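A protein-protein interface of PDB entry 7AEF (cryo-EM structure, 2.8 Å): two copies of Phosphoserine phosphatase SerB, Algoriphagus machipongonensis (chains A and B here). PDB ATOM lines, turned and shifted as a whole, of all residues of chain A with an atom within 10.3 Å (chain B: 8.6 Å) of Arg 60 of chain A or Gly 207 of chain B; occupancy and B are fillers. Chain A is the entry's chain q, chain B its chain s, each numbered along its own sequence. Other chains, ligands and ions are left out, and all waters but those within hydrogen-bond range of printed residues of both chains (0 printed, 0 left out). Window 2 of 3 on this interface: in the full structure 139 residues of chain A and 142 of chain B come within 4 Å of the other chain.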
ATOM      1  N   ASP A  54      22.167   6.274  11.980  1.00  0.00           N
ATOM      2  CA  ASP A  54      21.060   6.703  12.844  1.00  0.00           C
ATOM      3  C   ASP A  54      20.486   5.592  13.706  1.00  0.00           C
ATOM      4  O   ASP A  54      20.627   4.418  13.390  1.00  0.00           O
ATOM      5  CB  ASP A  54      19.906   7.292  12.018  1.00  0.00           C
ATOM      6  CG  ASP A  54      18.964   8.215  12.861  1.00  0.00           C
ATOM      7  OD1 ASP A  54      19.243   8.426  14.026  1.00  0.00           O
ATOM      8  OD2 ASP A  54      17.946   8.639  12.358  1.00  0.00           O
ATOM      9  N   GLY A  55      19.783   5.989  14.750  1.00  0.00           N
ATOM     10  CA  GLY A  55      19.063   5.091  15.640  1.00  0.00           C
ATOM     11  C   GLY A  55      19.793   4.844  16.948  1.00  0.00           C
ATOM     12  O   GLY A  55      21.005   4.624  16.969  1.00  0.00           O
ATOM     13  N   ASP A  56      19.053   4.853  18.052  1.00  0.00           N
ATOM     14  CA  ASP A  56      19.659   4.619  19.364  1.00  0.00           C
ATOM     15  C   ASP A  56      18.744   3.818  20.283  1.00  0.00           C
ATOM     16  O   ASP A  56      17.656   4.271  20.678  1.00  0.00           O
ATOM     17  CB  ASP A  56      20.089   5.908  20.063  1.00  0.00           C
ATOM     18  CG  ASP A  56      20.866   5.585  21.353  1.00  0.00           C
ATOM     19  OD1 ASP A  56      20.919   4.397  21.675  1.00  0.00           O
ATOM     20  OD2 ASP A  56      21.409   6.461  21.983  1.00  0.00           O
ATOM     21  N   ALA A  57      19.170   2.593  20.574  1.00  0.00           N
ATOM     22  CA  ALA A  57      18.443   1.612  21.379  1.00  0.00           C
ATOM     23  C   ALA A  57      18.171   2.093  22.788  1.00  0.00           C
ATOM     24  O   ALA A  57      17.268   1.590  23.453  1.00  0.00           O
ATOM     25  CB  ALA A  57      19.220   0.321  21.457  1.00  0.00           C
ATOM     26  N   ALA A  58      18.993   3.013  23.278  1.00  0.00           N
ATOM     27  CA  ALA A  58      18.838   3.539  24.619  1.00  0.00           C
ATOM     28  C   ALA A  58      17.783   4.636  24.685  1.00  0.00           C
ATOM     29  O   ALA A  58      17.416   5.070  25.774  1.00  0.00           O
ATOM     30  CB  ALA A  58      20.154   4.079  25.114  1.00  0.00           C
ATOM     31  N   GLU A  59      17.318   5.119  23.531  1.00  0.00           N
ATOM     32  CA  GLU A  59      16.320   6.172  23.476  1.00  0.00           C
ATOM     33  C   GLU A  59      15.045   5.614  22.909  1.00  0.00           C
ATOM     34  O   GLU A  59      13.955   6.099  23.199  1.00  0.00           O
ATOM     35  CB  GLU A  59      16.777   7.345  22.630  1.00  0.00           C
ATOM     36  CG  GLU A  59      17.972   8.075  23.169  1.00  0.00           C
ATOM     37  CD  GLU A  59      18.311   9.275  22.353  1.00  0.00           C
ATOM     38  OE1 GLU A  59      17.690   9.468  21.333  1.00  0.00           O
ATOM     39  OE2 GLU A  59      19.159  10.036  22.746  1.00  0.00           O
ATOM     40  N   ARG A  60      15.199   4.545  22.158  1.00  0.00           N
ATOM     41  CA  ARG A  60      14.067   3.997  21.508  1.00  0.00           C
ATOM     42  C   ARG A  60      13.627   4.871  20.337  1.00  0.00           C
ATOM     43  O   ARG A  60      12.469   5.180  20.246  1.00  0.00           O
ATOM     44  CB  ARG A  60      12.927   3.915  22.508  1.00  0.00           C
ATOM     45  CG  ARG A  60      12.794   2.622  23.275  1.00  0.00           C
ATOM     46  CD  ARG A  60      13.677   2.598  24.489  1.00  0.00           C
ATOM     47  NE  ARG A  60      13.262   1.572  25.426  1.00  0.00           N
ATOM     48  CZ  ARG A  60      14.097   0.809  26.112  1.00  0.00           C
ATOM     49  NH1 ARG A  60      15.401   0.940  25.943  1.00  0.00           N
ATOM     50  NH2 ARG A  60      13.624  -0.087  26.960  1.00  0.00           N
ATOM     51  N   ASP A  61      14.538   5.380  19.507  1.00  0.00           N
ATOM     52  CA  ASP A  61      14.084   6.149  18.349  1.00  0.00           C
ATOM     53  C   ASP A  61      15.156   6.376  17.270  1.00  0.00           C
ATOM     54  O   ASP A  61      16.326   6.025  17.445  1.00  0.00           O
ATOM     55  CB  ASP A  61      13.547   7.515  18.830  1.00  0.00           C
ATOM     56  CG  ASP A  61      12.504   8.125  17.890  1.00  0.00           C
ATOM     57  OD1 ASP A  61      12.253   7.500  16.892  1.00  0.00           O
ATOM     58  OD2 ASP A  61      12.014   9.200  18.119  1.00  0.00           O
ATOM     59  N   PHE A  62      14.728   7.017  16.171  1.00  0.00           N
ATOM     60  CA  PHE A  62      15.524   7.477  15.017  1.00  0.00           C
ATOM     61  C   PHE A  62      15.310   8.953  14.673  1.00  0.00           C
ATOM     62  O   PHE A  62      14.384   9.305  13.934  1.00  0.00           O
ATOM     63  CB  PHE A  62      15.213   6.664  13.762  1.00  0.00           C
ATOM     64  CG  PHE A  62      15.671   5.261  13.742  1.00  0.00           C
ATOM     65  CD1 PHE A  62      15.045   4.258  14.412  1.00  0.00           C
ATOM     66  CD2 PHE A  62      16.753   4.951  12.966  1.00  0.00           C
ATOM     67  CE1 PHE A  62      15.515   2.977  14.324  1.00  0.00           C
ATOM     68  CE2 PHE A  62      17.221   3.682  12.864  1.00  0.00           C
ATOM     69  CZ  PHE A  62      16.608   2.698  13.544  1.00  0.00           C
ATOM     70  N   LYS A  63      16.193   9.809  15.158  1.00  0.00           N
ATOM     71  CA  LYS A  63      16.051  11.248  14.974  1.00  0.00           C
ATOM     72  C   LYS A  63      16.116  11.781  13.548  1.00  0.00           C
ATOM     73  O   LYS A  63      15.489  12.799  13.265  1.00  0.00           O
ATOM     74  CB  LYS A  63      17.071  11.997  15.810  1.00  0.00           C
ATOM     75  CG  LYS A  63      16.779  11.984  17.280  1.00  0.00           C
ATOM     76  CD  LYS A  63      17.776  12.851  18.040  1.00  0.00           C
ATOM     77  CE  LYS A  63      17.397  13.001  19.522  1.00  0.00           C
ATOM     78  NZ  LYS A  63      17.543  11.729  20.279  1.00  0.00           N
ATOM     79  N   ASN A  66      12.816  10.978  11.704  1.00  0.00           N
ATOM     80  CA  ASN A  66      11.744  11.844  12.185  1.00  0.00           C
ATOM     81  C   ASN A  66      11.800  13.286  11.663  1.00  0.00           C
ATOM     82  O   ASN A  66      10.870  14.059  11.909  1.00  0.00           O
ATOM     83  CB  ASN A  66      11.784  11.970  13.687  1.00  0.00           C
ATOM     84  CG  ASN A  66      11.408  10.785  14.450  1.00  0.00           C
ATOM     85  OD1 ASN A  66      10.797   9.841  13.950  1.00  0.00           O
ATOM     86  ND2 ASN A  66      11.764  10.836  15.708  1.00  0.00           N
ATOM     87  N   LEU A  99      14.983   1.690   6.715  1.00  0.00           N
ATOM     88  CA  LEU A  99      15.775   1.500   7.934  1.00  0.00           C
ATOM     89  C   LEU A  99      16.310   0.090   8.026  1.00  0.00           C
ATOM     90  O   LEU A  99      15.624  -0.858   7.650  1.00  0.00           O
ATOM     91  CB  LEU A  99      14.956   1.779   9.194  1.00  0.00           C
ATOM     92  CG  LEU A  99      14.334   3.164   9.346  1.00  0.00           C
ATOM     93  CD1 LEU A  99      13.542   3.191  10.611  1.00  0.00           C
ATOM     94  CD2 LEU A  99      15.402   4.226   9.385  1.00  0.00           C
ATOM     95  N   ILE A 101      18.333  -2.591  10.880  1.00  0.00           N
ATOM     96  CA  ILE A 101      18.882  -2.897  12.202  1.00  0.00           C
ATOM     97  C   ILE A 101      19.470  -4.304  12.272  1.00  0.00           C
ATOM     98  O   ILE A 101      18.810  -5.285  11.921  1.00  0.00           O
ATOM     99  CB  ILE A 101      17.816  -2.757  13.307  1.00  0.00           C
ATOM    100  CG1 ILE A 101      17.277  -1.326  13.332  1.00  0.00           C
ATOM    101  CG2 ILE A 101      18.417  -3.133  14.665  1.00  0.00           C
ATOM    102  CD1 ILE A 101      16.071  -1.127  14.218  1.00  0.00           C
ATOM    103  N   SER A 106      23.028   0.147  13.010  1.00  0.00           N
ATOM    104  CA  SER A 106      21.748   0.799  12.745  1.00  0.00           C
ATOM    105  C   SER A 106      21.911   1.975  11.780  1.00  0.00           C
ATOM    106  O   SER A 106      22.651   2.930  12.059  1.00  0.00           O
ATOM    107  CB  SER A 106      21.128   1.236  14.052  1.00  0.00           C
ATOM    108  OG  SER A 106      19.919   1.885  13.848  1.00  0.00           O
ATOM    109  N   ASN B   3       3.409  -4.576  28.906  1.00  0.00           N
ATOM    110  CA  ASN B   3       4.487  -3.593  29.037  1.00  0.00           C
ATOM    111  C   ASN B   3       5.668  -4.124  29.809  1.00  0.00           C
ATOM    112  O   ASN B   3       6.512  -3.386  30.227  1.00  0.00           O
ATOM    113  CB  ASN B   3       3.994  -2.397  29.825  1.00  0.00           C
ATOM    114  CG  ASN B   3       3.383  -1.349  28.963  1.00  0.00           C
ATOM    115  OD1 ASN B   3       2.175  -1.268  28.839  1.00  0.00           O
ATOM    116  ND2 ASN B   3       4.214  -0.534  28.359  1.00  0.00           N
ATOM    117  N   GLY B   5       8.364  -5.619  29.103  1.00  0.00           N
ATOM    118  CA  GLY B   5       9.703  -5.532  28.543  1.00  0.00           C
ATOM    119  C   GLY B   5      10.221  -6.866  28.029  1.00  0.00           C
ATOM    120  O   GLY B   5      11.370  -6.968  27.608  1.00  0.00           O
ATOM    121  N   VAL B 204       6.174  -5.795  20.457  1.00  0.00           N
ATOM    122  CA  VAL B 204       7.574  -6.044  20.177  1.00  0.00           C
ATOM    123  C   VAL B 204       8.294  -4.685  20.160  1.00  0.00           C
ATOM    124  O   VAL B 204       7.884  -3.771  19.442  1.00  0.00           O
ATOM    125  CB  VAL B 204       7.719  -6.863  18.875  1.00  0.00           C
ATOM    126  CG1 VAL B 204       9.124  -7.103  18.609  1.00  0.00           C
ATOM    127  CG2 VAL B 204       6.981  -8.206  19.003  1.00  0.00           C
ATOM    128  N   THR B 205       9.319  -4.547  21.012  1.00  0.00           N
ATOM    129  CA  THR B 205       9.989  -3.260  21.222  1.00  0.00           C
ATOM    130  C   THR B 205      11.475  -3.212  20.854  1.00  0.00           C
ATOM    131  O   THR B 205      12.293  -4.047  21.272  1.00  0.00           O
ATOM    132  CB  THR B 205       9.827  -2.834  22.702  1.00  0.00           C
ATOM    133  OG1 THR B 205       8.455  -2.730  23.009  1.00  0.00           O
ATOM    134  CG2 THR B 205      10.463  -1.489  22.959  1.00  0.00           C
ATOM    135  N   PHE B 206      11.859  -2.179  20.122  1.00  0.00           N
ATOM    136  CA  PHE B 206      13.258  -2.037  19.721  1.00  0.00           C
ATOM    137  C   PHE B 206      14.274  -2.079  20.838  1.00  0.00           C
ATOM    138  O   PHE B 206      15.267  -2.799  20.763  1.00  0.00           O
ATOM    139  CB  PHE B 206      13.488  -0.817  18.874  1.00  0.00           C
ATOM    140  CG  PHE B 206      14.925  -0.571  18.653  1.00  0.00           C
ATOM    141  CD1 PHE B 206      15.710  -1.475  17.987  1.00  0.00           C
ATOM    142  CD2 PHE B 206      15.497   0.586  19.093  1.00  0.00           C
ATOM    143  CE1 PHE B 206      17.043  -1.232  17.810  1.00  0.00           C
ATOM    144  CE2 PHE B 206      16.824   0.830  18.901  1.00  0.00           C
ATOM    145  CZ  PHE B 206      17.597  -0.083  18.268  1.00  0.00           C
ATOM    146  N   GLY B 207      14.063  -1.337  21.884  1.00  0.00           N
ATOM    147  CA  GLY B 207      15.050  -1.323  22.941  1.00  0.00           C
ATOM    148  C   GLY B 207      14.929  -2.479  23.941  1.00  0.00           C
ATOM    149  O   GLY B 207      15.602  -2.454  24.967  1.00  0.00           O
ATOM    150  N   ALA B 208      14.032  -3.455  23.714  1.00  0.00           N
ATOM    151  CA  ALA B 208      13.884  -4.522  24.696  1.00  0.00           C
ATOM    152  C   ALA B 208      13.785  -5.944  24.123  1.00  0.00           C
ATOM    153  O   ALA B 208      14.315  -6.871  24.733  1.00  0.00           O
ATOM    154  CB  ALA B 208      12.648  -4.253  25.525  1.00  0.00           C
ATOM    155  N   THR B 209      13.093  -6.148  22.991  1.00  0.00           N
ATOM    156  CA  THR B 209      12.861  -7.509  22.509  1.00  0.00           C
ATOM    157  C   THR B 209      13.290  -7.813  21.058  1.00  0.00           C
ATOM    158  O   THR B 209      13.438  -8.981  20.703  1.00  0.00           O
ATOM    159  CB  THR B 209      11.388  -7.932  22.717  1.00  0.00           C
ATOM    160  OG1 THR B 209      10.482  -7.107  21.978  1.00  0.00           O
ATOM    161  CG2 THR B 209      11.011  -7.837  24.176  1.00  0.00           C
ATOM    162  N   ILE B 210      13.525  -6.798  20.228  1.00  0.00           N
ATOM    163  CA  ILE B 210      13.899  -7.027  18.820  1.00  0.00           C
ATOM    164  C   ILE B 210      15.347  -7.466  18.602  1.00  0.00           C
ATOM    165  O   ILE B 210      16.274  -6.856  19.121  1.00  0.00           O
ATOM    166  CB  ILE B 210      13.622  -5.781  17.934  1.00  0.00           C
ATOM    167  CG1 ILE B 210      12.127  -5.537  17.873  1.00  0.00           C
ATOM    168  CG2 ILE B 210      14.214  -5.906  16.570  1.00  0.00           C
ATOM    169  CD1 ILE B 210      11.638  -4.272  17.149  1.00  0.00           C
ATOM    170  N   LEU B 211      15.538  -8.526  17.805  1.00  0.00           N
ATOM    171  CA  LEU B 211      16.863  -9.030  17.454  1.00  0.00           C
ATOM    172  C   LEU B 211      17.332  -8.412  16.132  1.00  0.00           C
ATOM    173  O   LEU B 211      18.482  -7.999  15.999  1.00  0.00           O
ATOM    174  CB  LEU B 211      16.810 -10.552  17.304  1.00  0.00           C
ATOM    175  CG  LEU B 211      16.429 -11.374  18.562  1.00  0.00           C
ATOM    176  CD1 LEU B 211      16.240 -12.827  18.171  1.00  0.00           C
ATOM    177  CD2 LEU B 211      17.507 -11.268  19.605  1.00  0.00           C
ATOM    178  N   GLU B 318       6.784  -1.005  18.583  1.00  0.00           N
ATOM    179  CA  GLU B 318       7.231   0.191  19.290  1.00  0.00           C
ATOM    180  C   GLU B 318       8.740   0.431  19.278  1.00  0.00           C
ATOM    181  O   GLU B 318       9.541  -0.504  19.226  1.00  0.00           O
ATOM    182  CB  GLU B 318       6.771   0.150  20.744  1.00  0.00           C
ATOM    183  CG  GLU B 318       5.270   0.209  20.933  1.00  0.00           C
ATOM    184  CD  GLU B 318       4.862   0.251  22.379  1.00  0.00           C
ATOM    185  OE1 GLU B 318       5.682  -0.051  23.205  1.00  0.00           O
ATOM    186  OE2 GLU B 318       3.749   0.633  22.667  1.00  0.00           O
ATOM    187  N   GLY B 319       9.110   1.707  19.389  1.00  0.00           N
ATOM    188  CA  GLY B 319      10.501   2.130  19.513  1.00  0.00           C
ATOM    189  C   GLY B 319      11.304   2.258  18.219  1.00  0.00           C
ATOM    190  O   GLY B 319      12.527   2.307  18.284  1.00  0.00           O
ATOM    191  N   VAL B 320      10.653   2.331  17.056  1.00  0.00           N
ATOM    192  CA  VAL B 320      11.390   2.416  15.791  1.00  0.00           C
ATOM    193  C   VAL B 320      11.145   3.716  15.022  1.00  0.00           C
ATOM    194  O   VAL B 320      11.378   3.789  13.821  1.00  0.00           O
ATOM    195  CB  VAL B 320      11.077   1.219  14.865  1.00  0.00           C
ATOM    196  CG1 VAL B 320      11.567  -0.088  15.481  1.00  0.00           C
ATOM    197  CG2 VAL B 320       9.599   1.131  14.624  1.00  0.00           C
ATOM    198  N   GLY B 321      10.660   4.729  15.713  1.00  0.00           N
ATOM    199  CA  GLY B 321      10.393   6.028  15.114  1.00  0.00           C
ATOM    200  C   GLY B 321       8.942   6.219  14.688  1.00  0.00           C
ATOM    201  O   GLY B 321       8.268   5.284  14.246  1.00  0.00           O
ATOM    202  N   ASP B 322       8.507   7.474  14.701  1.00  0.00           N
ATOM    203  CA  ASP B 322       7.138   7.877  14.375  1.00  0.00           C
ATOM    204  C   ASP B 322       6.685   7.474  12.986  1.00  0.00           C
ATOM    205  O   ASP B 322       5.496   7.352  12.720  1.00  0.00           O
ATOM    206  CB  ASP B 322       7.031   9.383  14.475  1.00  0.00           C
ATOM    207  CG  ASP B 322       7.130   9.904  15.884  1.00  0.00           C
ATOM    208  OD1 ASP B 322       6.987   9.153  16.814  1.00  0.00           O
ATOM    209  OD2 ASP B 322       7.380  11.069  16.020  1.00  0.00           O
ATOM    210  N   ASN B 325       6.082   3.355  13.820  1.00  0.00           N
ATOM    211  CA  ASN B 325       5.399   2.842  15.017  1.00  0.00           C
ATOM    212  C   ASN B 325       3.887   2.682  14.838  1.00  0.00           C
ATOM    213  O   ASN B 325       3.244   3.457  14.115  1.00  0.00           O
ATOM    214  CB  ASN B 325       5.635   3.737  16.216  1.00  0.00           C
ATOM    215  CG  ASN B 325       7.015   3.710  16.792  1.00  0.00           C
ATOM    216  OD1 ASN B 325       7.770   2.729  16.743  1.00  0.00           O
ATOM    217  ND2 ASN B 325       7.352   4.815  17.377  1.00  0.00           N
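Arg 60 of chain A touches just these residues of chain B: Gly 207 (3.5 Å) and Gly 319 (3.5 Å). Of chain A, only Ala 57 (3.7 Å) and Arg 60 (3.5 Å) come within 4 Å of Gly 207 of chain B. Printed residues of chain A within 4 Å of Phe 206 of chain B: Asp 56 (3.8 Å), Ala 57 (3.1 Å) and Ile 101 (3.7 Å). No residue of chain A comes within 4 Å of Ala 208 of chain B. Of chain A, only Arg 60 (3.5 Å) and Asp 61 (3.9 Å) come within 4 Å of Gly 319 of chain B. Printed residues of chain B within 4 Å of Ile 101 of chain A: Phe 206. Of the printed residues of chain A, Val 320 of chain B touches Phe 62 (3.7 Å) and Leu 99 (3.9 Å). The nearest residue of chain B that does not touch Arg 60 of chain A is Phe 206 of chain B (4.4 Å).
No position is printed for both chains. Of the 11 pairs that touch across the chains among the printed residues, none has its exchanged pair printed and touching as well.
Asp 56 of chain A touches Phe 206 of chain B. Phe 206 of chain B touches Ala 57 of chain A (CE2 to CA, 3.1 Å). Ala 57 of chain A touches Gly 207 of chain B. O of Gly 207 of chain B touches NH1 of Arg 60 of chain A (3.5 Å). Asp 61 of chain A touches Gly 319 of chain B (N to O, 3.9 Å). Val 320 of chain B touches Phe 62 of chain A. CD1 of Leu 99 of chain A touches O of Val 320 of chain B, at 3.9 Å. Ile 101 of chain A touches Phe 206 of chain B (CD1 to CE1, 3.7 Å).
The side-chain amide nitrogen (ND2) of Asn 325 of chain B lies close to the backbone carbonyl oxygen (O) of Gly 321 of chain B, 3.3 Å away. The backbone NH (N) of Gly 319 of chain B is in hydrogen-bond range of the side-chain amide oxygen (OD1) of Asn 325 of chain B (3.1 Å). The backbone carbonyl oxygen of Ala 57 of chain A lies within hydrogen-bond range of the guanidinium group of Arg 60 of chain A (3.2 Å). The backbone NH of Asp 56 of chain A sits at hydrogen-bond distance from the backbone carbonyl oxygen of Asp 61 of chain A (3.0 Å). N of Val 320 of chain B lies within hydrogen-bond range of OD1 of Asn 325 of chain B. The side-chain carboxylate (OD2) of Asp 61 of chain A lies within hydrogen-bond range of the side-chain amide nitrogen (ND2) of Asn 66 of chain A (2.9 Å).
O of Arg 60 of chain A sits close to O of Gly 319 of chain B. OD1 of Asn 66 of chain A sits at hydrogen-bond distance from N of Asp 322 of chain B. The side-chain carboxylate of Asp 61 of chain A sits close to the backbone NH of Gly 321 of chain B, at 3.4 Å.
Of the 14 printed residues of chain A, 8 touch a printed residue of chain B. Hydrophobic or aromatic side chains of chain A within 4 Å of the printed part of chain B: Ala 57, Phe 62, Leu 99 and Ile 101. Among the printed residues, 11 pairs touch across the chains. Among the printed residues, no Asp or Glu carboxylate lies within 4 Å of a Lys or Arg side-chain nitrogen of the other chain.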
